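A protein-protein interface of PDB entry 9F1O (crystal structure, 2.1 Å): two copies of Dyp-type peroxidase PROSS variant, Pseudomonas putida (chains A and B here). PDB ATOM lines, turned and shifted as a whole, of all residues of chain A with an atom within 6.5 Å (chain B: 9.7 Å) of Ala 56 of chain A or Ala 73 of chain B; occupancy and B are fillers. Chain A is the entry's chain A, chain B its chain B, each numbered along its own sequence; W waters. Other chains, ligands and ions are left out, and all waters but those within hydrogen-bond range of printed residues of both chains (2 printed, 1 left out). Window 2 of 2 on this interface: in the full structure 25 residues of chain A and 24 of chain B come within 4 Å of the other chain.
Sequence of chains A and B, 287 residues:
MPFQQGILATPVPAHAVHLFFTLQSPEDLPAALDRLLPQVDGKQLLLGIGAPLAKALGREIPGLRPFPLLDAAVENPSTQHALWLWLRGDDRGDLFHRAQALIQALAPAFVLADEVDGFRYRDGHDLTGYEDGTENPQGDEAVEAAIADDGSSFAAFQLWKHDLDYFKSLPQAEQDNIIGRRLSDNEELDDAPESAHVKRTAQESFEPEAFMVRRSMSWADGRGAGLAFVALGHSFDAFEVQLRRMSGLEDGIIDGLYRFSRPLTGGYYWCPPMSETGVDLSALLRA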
ATOM      1  N   LEU A  23      15.671  31.952 -28.267  1.00  0.00           N
ATOM      2  CA  LEU A  23      16.576  32.864 -27.574  1.00  0.00           C
ATOM      3  C   LEU A  23      17.923  32.854 -28.287  1.00  0.00           C
ATOM      4  O   LEU A  23      18.653  31.859 -28.239  1.00  0.00           O
ATOM      5  CB  LEU A  23      16.727  32.460 -26.110  1.00  0.00           C
ATOM      6  CG  LEU A  23      17.667  33.334 -25.281  1.00  0.00           C
ATOM      7  CD1 LEU A  23      17.049  34.703 -25.031  1.00  0.00           C
ATOM      8  CD2 LEU A  23      18.026  32.656 -23.974  1.00  0.00           C
ATOM      9  N   PRO A  26      21.230  36.071 -25.301  1.00  0.00           N
ATOM     10  CA  PRO A  26      20.900  36.110 -23.866  1.00  0.00           C
ATOM     11  C   PRO A  26      21.265  37.418 -23.182  1.00  0.00           C
ATOM     12  O   PRO A  26      20.618  37.790 -22.194  1.00  0.00           O
ATOM     13  CB  PRO A  26      21.705  34.937 -23.292  1.00  0.00           C
ATOM     14  CG  PRO A  26      21.930  34.020 -24.454  1.00  0.00           C
ATOM     15  CD  PRO A  26      22.073  34.915 -25.649  1.00  0.00           C
ATOM     16  N   LEU A  29      18.362  39.813 -22.985  1.00  0.00           N
ATOM     17  CA  LEU A  29      17.125  39.319 -22.386  1.00  0.00           C
ATOM     18  C   LEU A  29      16.493  40.279 -21.379  1.00  0.00           C
ATOM     19  O   LEU A  29      15.258  40.423 -21.411  1.00  0.00           O
ATOM     20  CB  LEU A  29      17.387  37.953 -21.738  1.00  0.00           C
ATOM     21  CG  LEU A  29      16.223  37.247 -21.038  1.00  0.00           C
ATOM     22  CD1 LEU A  29      15.085  36.982 -22.009  1.00  0.00           C
ATOM     23  CD2 LEU A  29      16.697  35.950 -20.395  1.00  0.00           C
ATOM     24  N   ALA A  51      11.668  25.058 -21.813  1.00  0.00           N
ATOM     25  CA  ALA A  51      12.882  24.547 -21.180  1.00  0.00           C
ATOM     26  C   ALA A  51      14.170  25.227 -21.636  1.00  0.00           C
ATOM     27  O   ALA A  51      15.038  25.462 -20.779  1.00  0.00           O
ATOM     28  CB  ALA A  51      12.974  23.029 -21.400  1.00  0.00           C
ATOM     29  N   PRO A  52      14.383  25.541 -22.924  1.00  0.00           N
ATOM     30  CA  PRO A  52      15.643  26.213 -23.296  1.00  0.00           C
ATOM     31  C   PRO A  52      15.880  27.521 -22.562  1.00  0.00           C
ATOM     32  O   PRO A  52      17.028  27.833 -22.219  1.00  0.00           O
ATOM     33  CB  PRO A  52      15.489  26.429 -24.807  1.00  0.00           C
ATOM     34  CG  PRO A  52      14.573  25.347 -25.245  1.00  0.00           C
ATOM     35  CD  PRO A  52      13.602  25.164 -24.118  1.00  0.00           C
ATOM     36  N   LEU A  53      14.826  28.304 -22.316  1.00  0.00           N
ATOM     37  CA  LEU A  53      15.001  29.570 -21.610  1.00  0.00           C
ATOM     38  C   LEU A  53      15.416  29.341 -20.163  1.00  0.00           C
ATOM     39  O   LEU A  53      16.305  30.031 -19.650  1.00  0.00           O
ATOM     40  CB  LEU A  53      13.714  30.395 -21.679  1.00  0.00           C
ATOM     41  CG  LEU A  53      13.755  31.793 -21.052  1.00  0.00           C
ATOM     42  CD1 LEU A  53      14.948  32.587 -21.571  1.00  0.00           C
ATOM     43  CD2 LEU A  53      12.450  32.538 -21.312  1.00  0.00           C
ATOM     44  N   ALA A  54      14.783  28.376 -19.489  1.00  0.00           N
ATOM     45  CA  ALA A  54      15.203  28.020 -18.138  1.00  0.00           C
ATOM     46  C   ALA A  54      16.629  27.487 -18.133  1.00  0.00           C
ATOM     47  O   ALA A  54      17.422  27.814 -17.243  1.00  0.00           O
ATOM     48  CB  ALA A  54      14.239  26.995 -17.541  1.00  0.00           C
ATOM     49  N   LYS A  55      16.969  26.652 -19.118  1.00  0.00           N
ATOM     50  CA  LYS A  55      18.331  26.141 -19.230  1.00  0.00           C
ATOM     51  C   LYS A  55      19.329  27.275 -19.439  1.00  0.00           C
ATOM     52  O   LYS A  55      20.443  27.241 -18.903  1.00  0.00           O
ATOM     53  CB  LYS A  55      18.410  25.135 -20.377  1.00  0.00           C
ATOM     54  CG  LYS A  55      19.415  24.022 -20.167  1.00  0.00           C
ATOM     55  CD  LYS A  55      19.037  23.193 -18.949  1.00  0.00           C
ATOM     56  CE  LYS A  55      19.583  21.781 -19.042  1.00  0.00           C
ATOM     57  NZ  LYS A  55      21.054  21.758 -19.263  1.00  0.00           N
ATOM     58  N   ALA A  56      18.948  28.287 -20.224  1.00  0.00           N
ATOM     59  CA  ALA A  56      19.850  29.399 -20.506  1.00  0.00           C
ATOM     60  C   ALA A  56      20.139  30.236 -19.265  1.00  0.00           C
ATOM     61  O   ALA A  56      21.210  30.845 -19.168  1.00  0.00           O
ATOM     62  CB  ALA A  56      19.264  30.279 -21.608  1.00  0.00           C
ATOM     63  N   LEU A  57      19.204  30.293 -18.321  1.00  0.00           N
ATOM     64  CA  LEU A  57      19.394  31.042 -17.088  1.00  0.00           C
ATOM     65  C   LEU A  57      19.905  30.183 -15.941  1.00  0.00           C
ATOM     66  O   LEU A  57      20.025  30.682 -14.819  1.00  0.00           O
ATOM     67  CB  LEU A  57      18.086  31.728 -16.678  1.00  0.00           C
ATOM     68  CG  LEU A  57      17.569  32.784 -17.657  1.00  0.00           C
ATOM     69  CD1 LEU A  57      16.192  33.289 -17.250  1.00  0.00           C
ATOM     70  CD2 LEU A  57      18.555  33.936 -17.774  1.00  0.00           C
ATOM     71  N   GLY A  58      20.208  28.911 -16.189  1.00  0.00           N
ATOM     72  CA  GLY A  58      20.671  28.043 -15.123  1.00  0.00           C
ATOM     73  C   GLY A  58      19.630  27.786 -14.059  1.00  0.00           C
ATOM     74  O   GLY A  58      19.981  27.488 -12.912  1.00  0.00           O
ATOM     75  N   ARG A  59      18.354  27.890 -14.411  1.00  0.00           N
ATOM     76  CA  ARG A  59      17.247  27.723 -13.484  1.00  0.00           C
ATOM     77  C   ARG A  59      16.471  26.465 -13.842  1.00  0.00           C
ATOM     78  O   ARG A  59      16.215  26.198 -15.021  1.00  0.00           O
ATOM     79  CB  ARG A  59      16.307  28.931 -13.544  1.00  0.00           C
ATOM     80  CG  ARG A  59      16.727  30.139 -12.724  1.00  0.00           C
ATOM     81  CD  ARG A  59      16.245  30.022 -11.288  1.00  0.00           C
ATOM     82  NE  ARG A  59      16.728  31.114 -10.450  1.00  0.00           N
ATOM     83  CZ  ARG A  59      16.247  31.395  -9.243  1.00  0.00           C
ATOM     84  NH1 ARG A  59      15.258  30.673  -8.733  1.00  0.00           N
ATOM     85  NH2 ARG A  59      16.746  32.407  -8.548  1.00  0.00           N
ATOM     86  N   LEU B  70      17.885  16.880 -27.082  1.00  0.00           N
ATOM     87  CA  LEU B  70      18.941  17.560 -26.342  1.00  0.00           C
ATOM     88  C   LEU B  70      18.315  18.664 -25.497  1.00  0.00           C
ATOM     89  O   LEU B  70      17.814  19.659 -26.031  1.00  0.00           O
ATOM     90  CB  LEU B  70      19.996  18.125 -27.290  1.00  0.00           C
ATOM     91  CG  LEU B  70      21.164  17.213 -27.684  1.00  0.00           C
ATOM     92  CD1 LEU B  70      20.685  15.903 -28.289  1.00  0.00           C
ATOM     93  CD2 LEU B  70      22.106  17.930 -28.639  1.00  0.00           C
ATOM     94  N   ASP B  71      18.350  18.485 -24.175  1.00  0.00           N
ATOM     95  CA  ASP B  71      17.793  19.456 -23.235  1.00  0.00           C
ATOM     96  C   ASP B  71      18.858  20.513 -22.958  1.00  0.00           C
ATOM     97  O   ASP B  71      19.554  20.495 -21.943  1.00  0.00           O
ATOM     98  CB  ASP B  71      17.336  18.760 -21.960  1.00  0.00           C
ATOM     99  CG  ASP B  71      16.514  19.660 -21.058  1.00  0.00           C
ATOM    100  OD1 ASP B  71      16.319  20.847 -21.400  1.00  0.00           O
ATOM    101  OD2 ASP B  71      16.054  19.176 -20.004  1.00  0.00           O
ATOM    102  N   ALA B  72      18.986  21.448 -23.892  1.00  0.00           N
ATOM    103  CA  ALA B  72      20.047  22.446 -23.867  1.00  0.00           C
ATOM    104  C   ALA B  72      19.451  23.850 -23.901  1.00  0.00           C
ATOM    105  O   ALA B  72      18.234  24.035 -23.997  1.00  0.00           O
ATOM    106  CB  ALA B  72      21.012  22.238 -25.038  1.00  0.00           C
ATOM    107  N   ALA B  73      20.332  24.847 -23.818  1.00  0.00           N
ATOM    108  CA  ALA B  73      19.945  26.245 -23.963  1.00  0.00           C
ATOM    109  C   ALA B  73      19.846  26.685 -25.417  1.00  0.00           C
ATOM    110  O   ALA B  73      19.506  27.845 -25.676  1.00  0.00           O
ATOM    111  CB  ALA B  73      20.935  27.148 -23.221  1.00  0.00           C
ATOM    112  N   VAL B  74      20.133  25.796 -26.365  1.00  0.00           N
ATOM    113  CA  VAL B  74      19.896  26.037 -27.779  1.00  0.00           C
ATOM    114  C   VAL B  74      18.964  24.946 -28.288  1.00  0.00           C
ATOM    115  O   VAL B  74      18.762  23.917 -27.640  1.00  0.00           O
ATOM    116  CB  VAL B  74      21.201  26.077 -28.595  1.00  0.00           C
ATOM    117  CG1 VAL B  74      22.043  27.265 -28.167  1.00  0.00           C
ATOM    118  CG2 VAL B  74      21.971  24.777 -28.422  1.00  0.00           C
ATOM    119  N   GLU B  75      18.397  25.178 -29.468  1.00  0.00           N
ATOM    120  CA  GLU B  75      17.302  24.365 -29.980  1.00  0.00           C
ATOM    121  C   GLU B  75      17.799  23.473 -31.110  1.00  0.00           C
ATOM    122  O   GLU B  75      18.266  23.968 -32.141  1.00  0.00           O
ATOM    123  CB  GLU B  75      16.147  25.250 -30.452  1.00  0.00           C
ATOM    124  CG  GLU B  75      15.520  26.063 -29.330  1.00  0.00           C
ATOM    125  CD  GLU B  75      14.469  27.033 -29.827  1.00  0.00           C
ATOM    126  OE1 GLU B  75      14.005  26.872 -30.972  1.00  0.00           O
ATOM    127  OE2 GLU B  75      14.111  27.959 -29.068  1.00  0.00           O
ATOM    128  N   ASN B  76      17.698  22.161 -30.905  1.00  0.00           N
ATOM    129  CA  ASN B  76      17.959  21.162 -31.940  1.00  0.00           C
ATOM    130  C   ASN B  76      16.723  20.279 -31.999  1.00  0.00           C
ATOM    131  O   ASN B  76      16.618  19.287 -31.262  1.00  0.00           O
ATOM    132  CB  ASN B  76      19.214  20.350 -31.633  1.00  0.00           C
ATOM    133  CG  ASN B  76      20.460  21.208 -31.562  1.00  0.00           C
ATOM    134  OD1 ASN B  76      21.032  21.579 -32.587  1.00  0.00           O
ATOM    135  ND2 ASN B  76      20.891  21.523 -30.346  1.00  0.00           N
ATOM    136  N   LEU B 243      27.391  17.305 -31.634  1.00  0.00           N
ATOM    137  CA  LEU B 243      26.226  18.160 -31.434  1.00  0.00           C
ATOM    138  C   LEU B 243      26.020  18.476 -29.958  1.00  0.00           C
ATOM    139  O   LEU B 243      25.650  19.601 -29.602  1.00  0.00           O
ATOM    140  CB  LEU B 243      24.978  17.504 -32.024  1.00  0.00           C
ATOM    141  CG  LEU B 243      23.736  18.399 -32.012  1.00  0.00           C
ATOM    142  CD1 LEU B 243      23.907  19.554 -32.988  1.00  0.00           C
ATOM    143  CD2 LEU B 243      22.475  17.606 -32.326  1.00  0.00           C
ATOM    144  N   ARG B 244      26.245  17.492 -29.086  1.00  0.00           N
ATOM    145  CA  ARG B 244      26.101  17.733 -27.655  1.00  0.00           C
ATOM    146  C   ARG B 244      27.124  18.748 -27.159  1.00  0.00           C
ATOM    147  O   ARG B 244      26.816  19.572 -26.290  1.00  0.00           O
ATOM    148  CB  ARG B 244      26.212  16.419 -26.882  1.00  0.00           C
ATOM    149  CG  ARG B 244      25.053  15.471 -27.140  1.00  0.00           C
ATOM    150  CD  ARG B 244      25.221  14.154 -26.404  1.00  0.00           C
ATOM    151  NE  ARG B 244      25.341  14.347 -24.963  1.00  0.00           N
ATOM    152  CZ  ARG B 244      24.306  14.510 -24.146  1.00  0.00           C
ATOM    153  NH1 ARG B 244      23.070  14.500 -24.628  1.00  0.00           N
ATOM    154  NH2 ARG B 244      24.504  14.679 -22.845  1.00  0.00           N
ATOM    155  N   MET B 246      28.459  21.106 -29.123  1.00  0.00           N
ATOM    156  CA  MET B 246      27.999  22.363 -29.706  1.00  0.00           C
ATOM    157  C   MET B 246      26.872  22.981 -28.892  1.00  0.00           C
ATOM    158  O   MET B 246      26.763  24.210 -28.818  1.00  0.00           O
ATOM    159  CB  MET B 246      27.543  22.139 -31.151  1.00  0.00           C
ATOM    160  CG  MET B 246      28.662  21.790 -32.119  1.00  0.00           C
ATOM    161  SD  MET B 246      28.053  21.338 -33.759  1.00  0.00           S
ATOM    162  CE  MET B 246      27.096  22.791 -34.185  1.00  0.00           C
ATOM    163  N   SER B 247      26.031  22.155 -28.276  1.00  0.00           N
ATOM    164  CA  SER B 247      24.876  22.626 -27.526  1.00  0.00           C
ATOM    165  C   SER B 247      25.200  22.966 -26.078  1.00  0.00           C
ATOM    166  O   SER B 247      24.284  23.269 -25.306  1.00  0.00           O
ATOM    167  CB  SER B 247      23.758  21.581 -27.572  1.00  0.00           C
ATOM    168  OG  SER B 247      23.419  21.263 -28.912  1.00  0.00           O
ATOM    169  N   GLY B 248      26.473  22.930 -25.692  1.00  0.00           N
ATOM    170  CA  GLY B 248      26.854  23.242 -24.330  1.00  0.00           C
ATOM    171  C   GLY B 248      26.636  22.135 -23.324  1.00  0.00           C
ATOM    172  O   GLY B 248      26.836  22.362 -22.126  1.00  0.00           O
ATOM    173  N   LEU B 249      26.224  20.946 -23.764  1.00  0.00           N
ATOM    174  CA  LEU B 249      25.948  19.858 -22.835  1.00  0.00           C
ATOM    175  C   LEU B 249      27.210  19.180 -22.318  1.00  0.00           C
ATOM    176  O   LEU B 249      27.125  18.402 -21.361  1.00  0.00           O
ATOM    177  CB  LEU B 249      25.042  18.816 -23.492  1.00  0.00           C
ATOM    178  CG  LEU B 249      23.664  19.313 -23.934  1.00  0.00           C
ATOM    179  CD1 LEU B 249      22.861  18.181 -24.557  1.00  0.00           C
ATOM    180  CD2 LEU B 249      22.914  19.932 -22.761  1.00  0.00           C
ATOM    181  N   GLY B 252      29.344  23.315 -20.933  1.00  0.00           N
ATOM    182  CA  GLY B 252      28.631  24.563 -20.757  1.00  0.00           C
ATOM    183  C   GLY B 252      28.909  25.628 -21.794  1.00  0.00           C
ATOM    184  O   GLY B 252      28.307  26.705 -21.724  1.00  0.00           O
ATOM    185  N   ILE B 253      29.800  25.374 -22.748  1.00  0.00           N
ATOM    186  CA  ILE B 253      30.169  26.347 -23.768  1.00  0.00           C
ATOM    187  C   ILE B 253      29.381  26.032 -25.033  1.00  0.00           C
ATOM    188  O   ILE B 253      29.466  24.917 -25.564  1.00  0.00           O
ATOM    189  CB  ILE B 253      31.682  26.331 -24.036  1.00  0.00           C
ATOM    190  CG1 ILE B 253      32.455  26.629 -22.748  1.00  0.00           C
ATOM    191  CG2 ILE B 253      32.041  27.345 -25.110  1.00  0.00           C
ATOM    192  CD1 ILE B 253      32.178  27.998 -22.169  1.00  0.00           C
ATOM    193  N   ILE B 254      28.612  27.008 -25.513  1.00  0.00           N
ATOM    194  CA  ILE B 254      27.737  26.831 -26.668  1.00  0.00           C
ATOM    195  C   ILE B 254      28.462  27.296 -27.923  1.00  0.00           C
ATOM    196  O   ILE B 254      29.169  28.311 -27.908  1.00  0.00           O
ATOM    197  CB  ILE B 254      26.411  27.594 -26.474  1.00  0.00           C
ATOM    198  CG1 ILE B 254      25.589  26.953 -25.354  1.00  0.00           C
ATOM    199  CG2 ILE B 254      25.607  27.636 -27.766  1.00  0.00           C
ATOM    200  CD1 ILE B 254      24.410  27.788 -24.907  1.00  0.00           C
ATOM    201  N   ASP B 255      28.291  26.545 -29.011  1.00  0.00           N
ATOM    202  CA  ASP B 255      28.865  26.925 -30.295  1.00  0.00           C
ATOM    203  C   ASP B 255      28.347  28.289 -30.736  1.00  0.00           C
ATOM    204  O   ASP B 255      27.159  28.595 -30.612  1.00  0.00           O
ATOM    205  CB  ASP B 255      28.535  25.868 -31.353  1.00  0.00           C
ATOM    206  CG  ASP B 255      29.383  26.008 -32.609  1.00  0.00           C
ATOM    207  OD1 ASP B 255      29.477  27.126 -33.157  1.00  0.00           O
ATOM    208  OD2 ASP B 255      29.958  24.991 -33.050  1.00  0.00           O
ATOM    209  N   TYR B 258      25.114  29.097 -33.096  1.00  0.00           N
ATOM    210  CA  TYR B 258      23.758  29.326 -32.615  1.00  0.00           C
ATOM    211  C   TYR B 258      23.426  30.804 -32.447  1.00  0.00           C
ATOM    212  O   TYR B 258      22.255  31.134 -32.228  1.00  0.00           O
ATOM    213  CB  TYR B 258      23.544  28.586 -31.294  1.00  0.00           C
ATOM    214  CG  TYR B 258      23.474  27.084 -31.453  1.00  0.00           C
ATOM    215  CD1 TYR B 258      22.321  26.469 -31.925  1.00  0.00           C
ATOM    216  CD2 TYR B 258      24.561  26.281 -31.134  1.00  0.00           C
ATOM    217  CE1 TYR B 258      22.251  25.094 -32.071  1.00  0.00           C
ATOM    218  CE2 TYR B 258      24.501  24.904 -31.278  1.00  0.00           C
ATOM    219  CZ  TYR B 258      23.343  24.317 -31.747  1.00  0.00           C
ATOM    220  OH  TYR B 258      23.277  22.949 -31.892  1.00  0.00           O
ATOM    221  N   ARG B 259      24.415  31.696 -32.542  1.00  0.00           N
ATOM    222  CA  ARG B 259      24.129  33.124 -32.444  1.00  0.00           C
ATOM    223  C   ARG B 259      23.433  33.651 -33.691  1.00  0.00           C
ATOM    224  O   ARG B 259      22.698  34.641 -33.612  1.00  0.00           O
ATOM    225  CB  ARG B 259      25.416  33.909 -32.194  1.00  0.00           C
ATOM    226  CG  ARG B 259      26.088  33.579 -30.881  1.00  0.00           C
ATOM    227  CD  ARG B 259      27.038  34.684 -30.462  1.00  0.00           C
ATOM    228  NE  ARG B 259      27.788  34.316 -29.269  1.00  0.00           N
ATOM    229  CZ  ARG B 259      29.082  34.015 -29.263  1.00  0.00           C
ATOM    230  NH1 ARG B 259      29.782  34.051 -30.389  1.00  0.00           N
ATOM    231  NH2 ARG B 259      29.676  33.685 -28.129  1.00  0.00           N
ATOM    232  N   SER B 261      22.403  31.113 -36.408  1.00  0.00           N
ATOM    233  CA  SER B 261      21.847  29.992 -37.150  1.00  0.00           C
ATOM    234  C   SER B 261      21.255  28.993 -36.169  1.00  0.00           C
ATOM    235  O   SER B 261      21.694  28.895 -35.020  1.00  0.00           O
ATOM    236  CB  SER B 261      22.907  29.314 -38.025  1.00  0.00           C
ATOM    237  OG  SER B 261      22.321  28.333 -38.862  1.00  0.00           O
ATOM    238  N   ARG B 262      20.249  28.254 -36.630  1.00  0.00           N
ATOM    239  CA  ARG B 262      19.605  27.237 -35.814  1.00  0.00           C
ATOM    240  C   ARG B 262      18.991  26.191 -36.729  1.00  0.00           C
ATOM    241  O   ARG B 262      18.515  26.529 -37.820  1.00  0.00           O
ATOM    242  CB  ARG B 262      18.525  27.833 -34.901  1.00  0.00           C
ATOM    243  CG  ARG B 262      17.415  28.527 -35.656  1.00  0.00           C
ATOM    244  CD  ARG B 262      16.444  29.218 -34.725  1.00  0.00           C
ATOM    245  NE  ARG B 262      15.346  29.807 -35.479  1.00  0.00           N
ATOM    246  CZ  ARG B 262      14.237  29.151 -35.807  1.00  0.00           C
ATOM    247  NH1 ARG B 262      14.076  27.890 -35.430  1.00  0.00           N
ATOM    248  NH2 ARG B 262      13.287  29.759 -36.502  1.00  0.00           N
HETATM  249  O   HOH W   1      15.937  29.228 -27.428  1.00  0.00           O
HETATM  250  O   HOH W   2      18.512  29.258 -27.902  1.00  0.00           O
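O of Asp 71 of chain B sits close to NZ of Lys 55 of chain A (3.3 Å).
Water W2 lies within hydrogen-bond range of the backbone carbonyl oxygen of Leu 23 of chain A (2.6 Å) and the backbone carbonyl oxygen of Ala 73 of chain B (2.8 Å).
Water W1 lies within hydrogen-bond range of OE2 of Glu 75 of chain B (2.8 Å) and N of Leu 23 of chain A (2.9 Å).
Printed residues of chain A that touch a printed residue of chain B: Ala 51, Pro 52, Lys 55 and Ala 56.
Hydrophobic or aromatic side chains of chain A within 4 Å of the printed part of chain B: Ala 51, Pro 52 and Ala 56.
Of the 21 printed residues of chain B, 3 touch a printed residue of chain A.
Hydrophobic or aromatic side chains of chain B within 4 Å of the printed part of chain A: Ala 73.
Along chain B the printed residues that touch a printed residue of chain A span positions 71 to 73.
Among the printed residues, no Asp or Glu carboxylate lies within 4 Å of a Lys or Arg side-chain nitrogen of the other chain.
CB of Ala 51 of chain A touches OD1 of Asp 71 of chain B, at 3.99 Å.
Pro 52 of chain A touches Ala 72 of chain B.
O of Pro 52 of chain A touches CA of Ala 73 of chain B, at 3.8 Å.
Lys 55 of chain A touches Ala 72 of chain B (CG to C, 3.7 Å).
Lys 55 of chain A touches Ala 73 of chain B.
Ala 73 of chain B touches Ala 56 of chain A.
Printed residues of chain B within 4 Å of Ala 51 of chain A: Asp 71.
Printed residues of chain B within 4 Å of Pro 52 of chain A: Ala 72 and Ala 73.
No residue of chain B comes within 4 Å of Ala 54 of chain A.
No residue of chain B comes within 4 Å of Leu 57 of chain A.
Printed residues of chain A within 4 Å of Asp 71 of chain B: Ala 51 and Lys 55.
Of the printed residues of chain A, Ala 72 of chain B touches Pro 52 and Lys 55.
Ala 73 of chain B touches just these residues of chain A: Pro 52 (3.8 Å), Lys 55 (3.9 Å) and Ala 56 (3.7 Å).
Ser 247 of chain B touches none of the printed residues of chain A.
The nearest residue of chain B that does not touch Ala 56 of chain A is Ala 72 of chain B (5.7 Å).
The nearest residue of chain A that does not touch Ala 73 of chain B is Leu 23 of chain A (4.8 Å).
No position is printed for both chains.
Of the 7 pairs that touch across the chains among the printed residues, none has its exchanged pair printed and touching as well.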
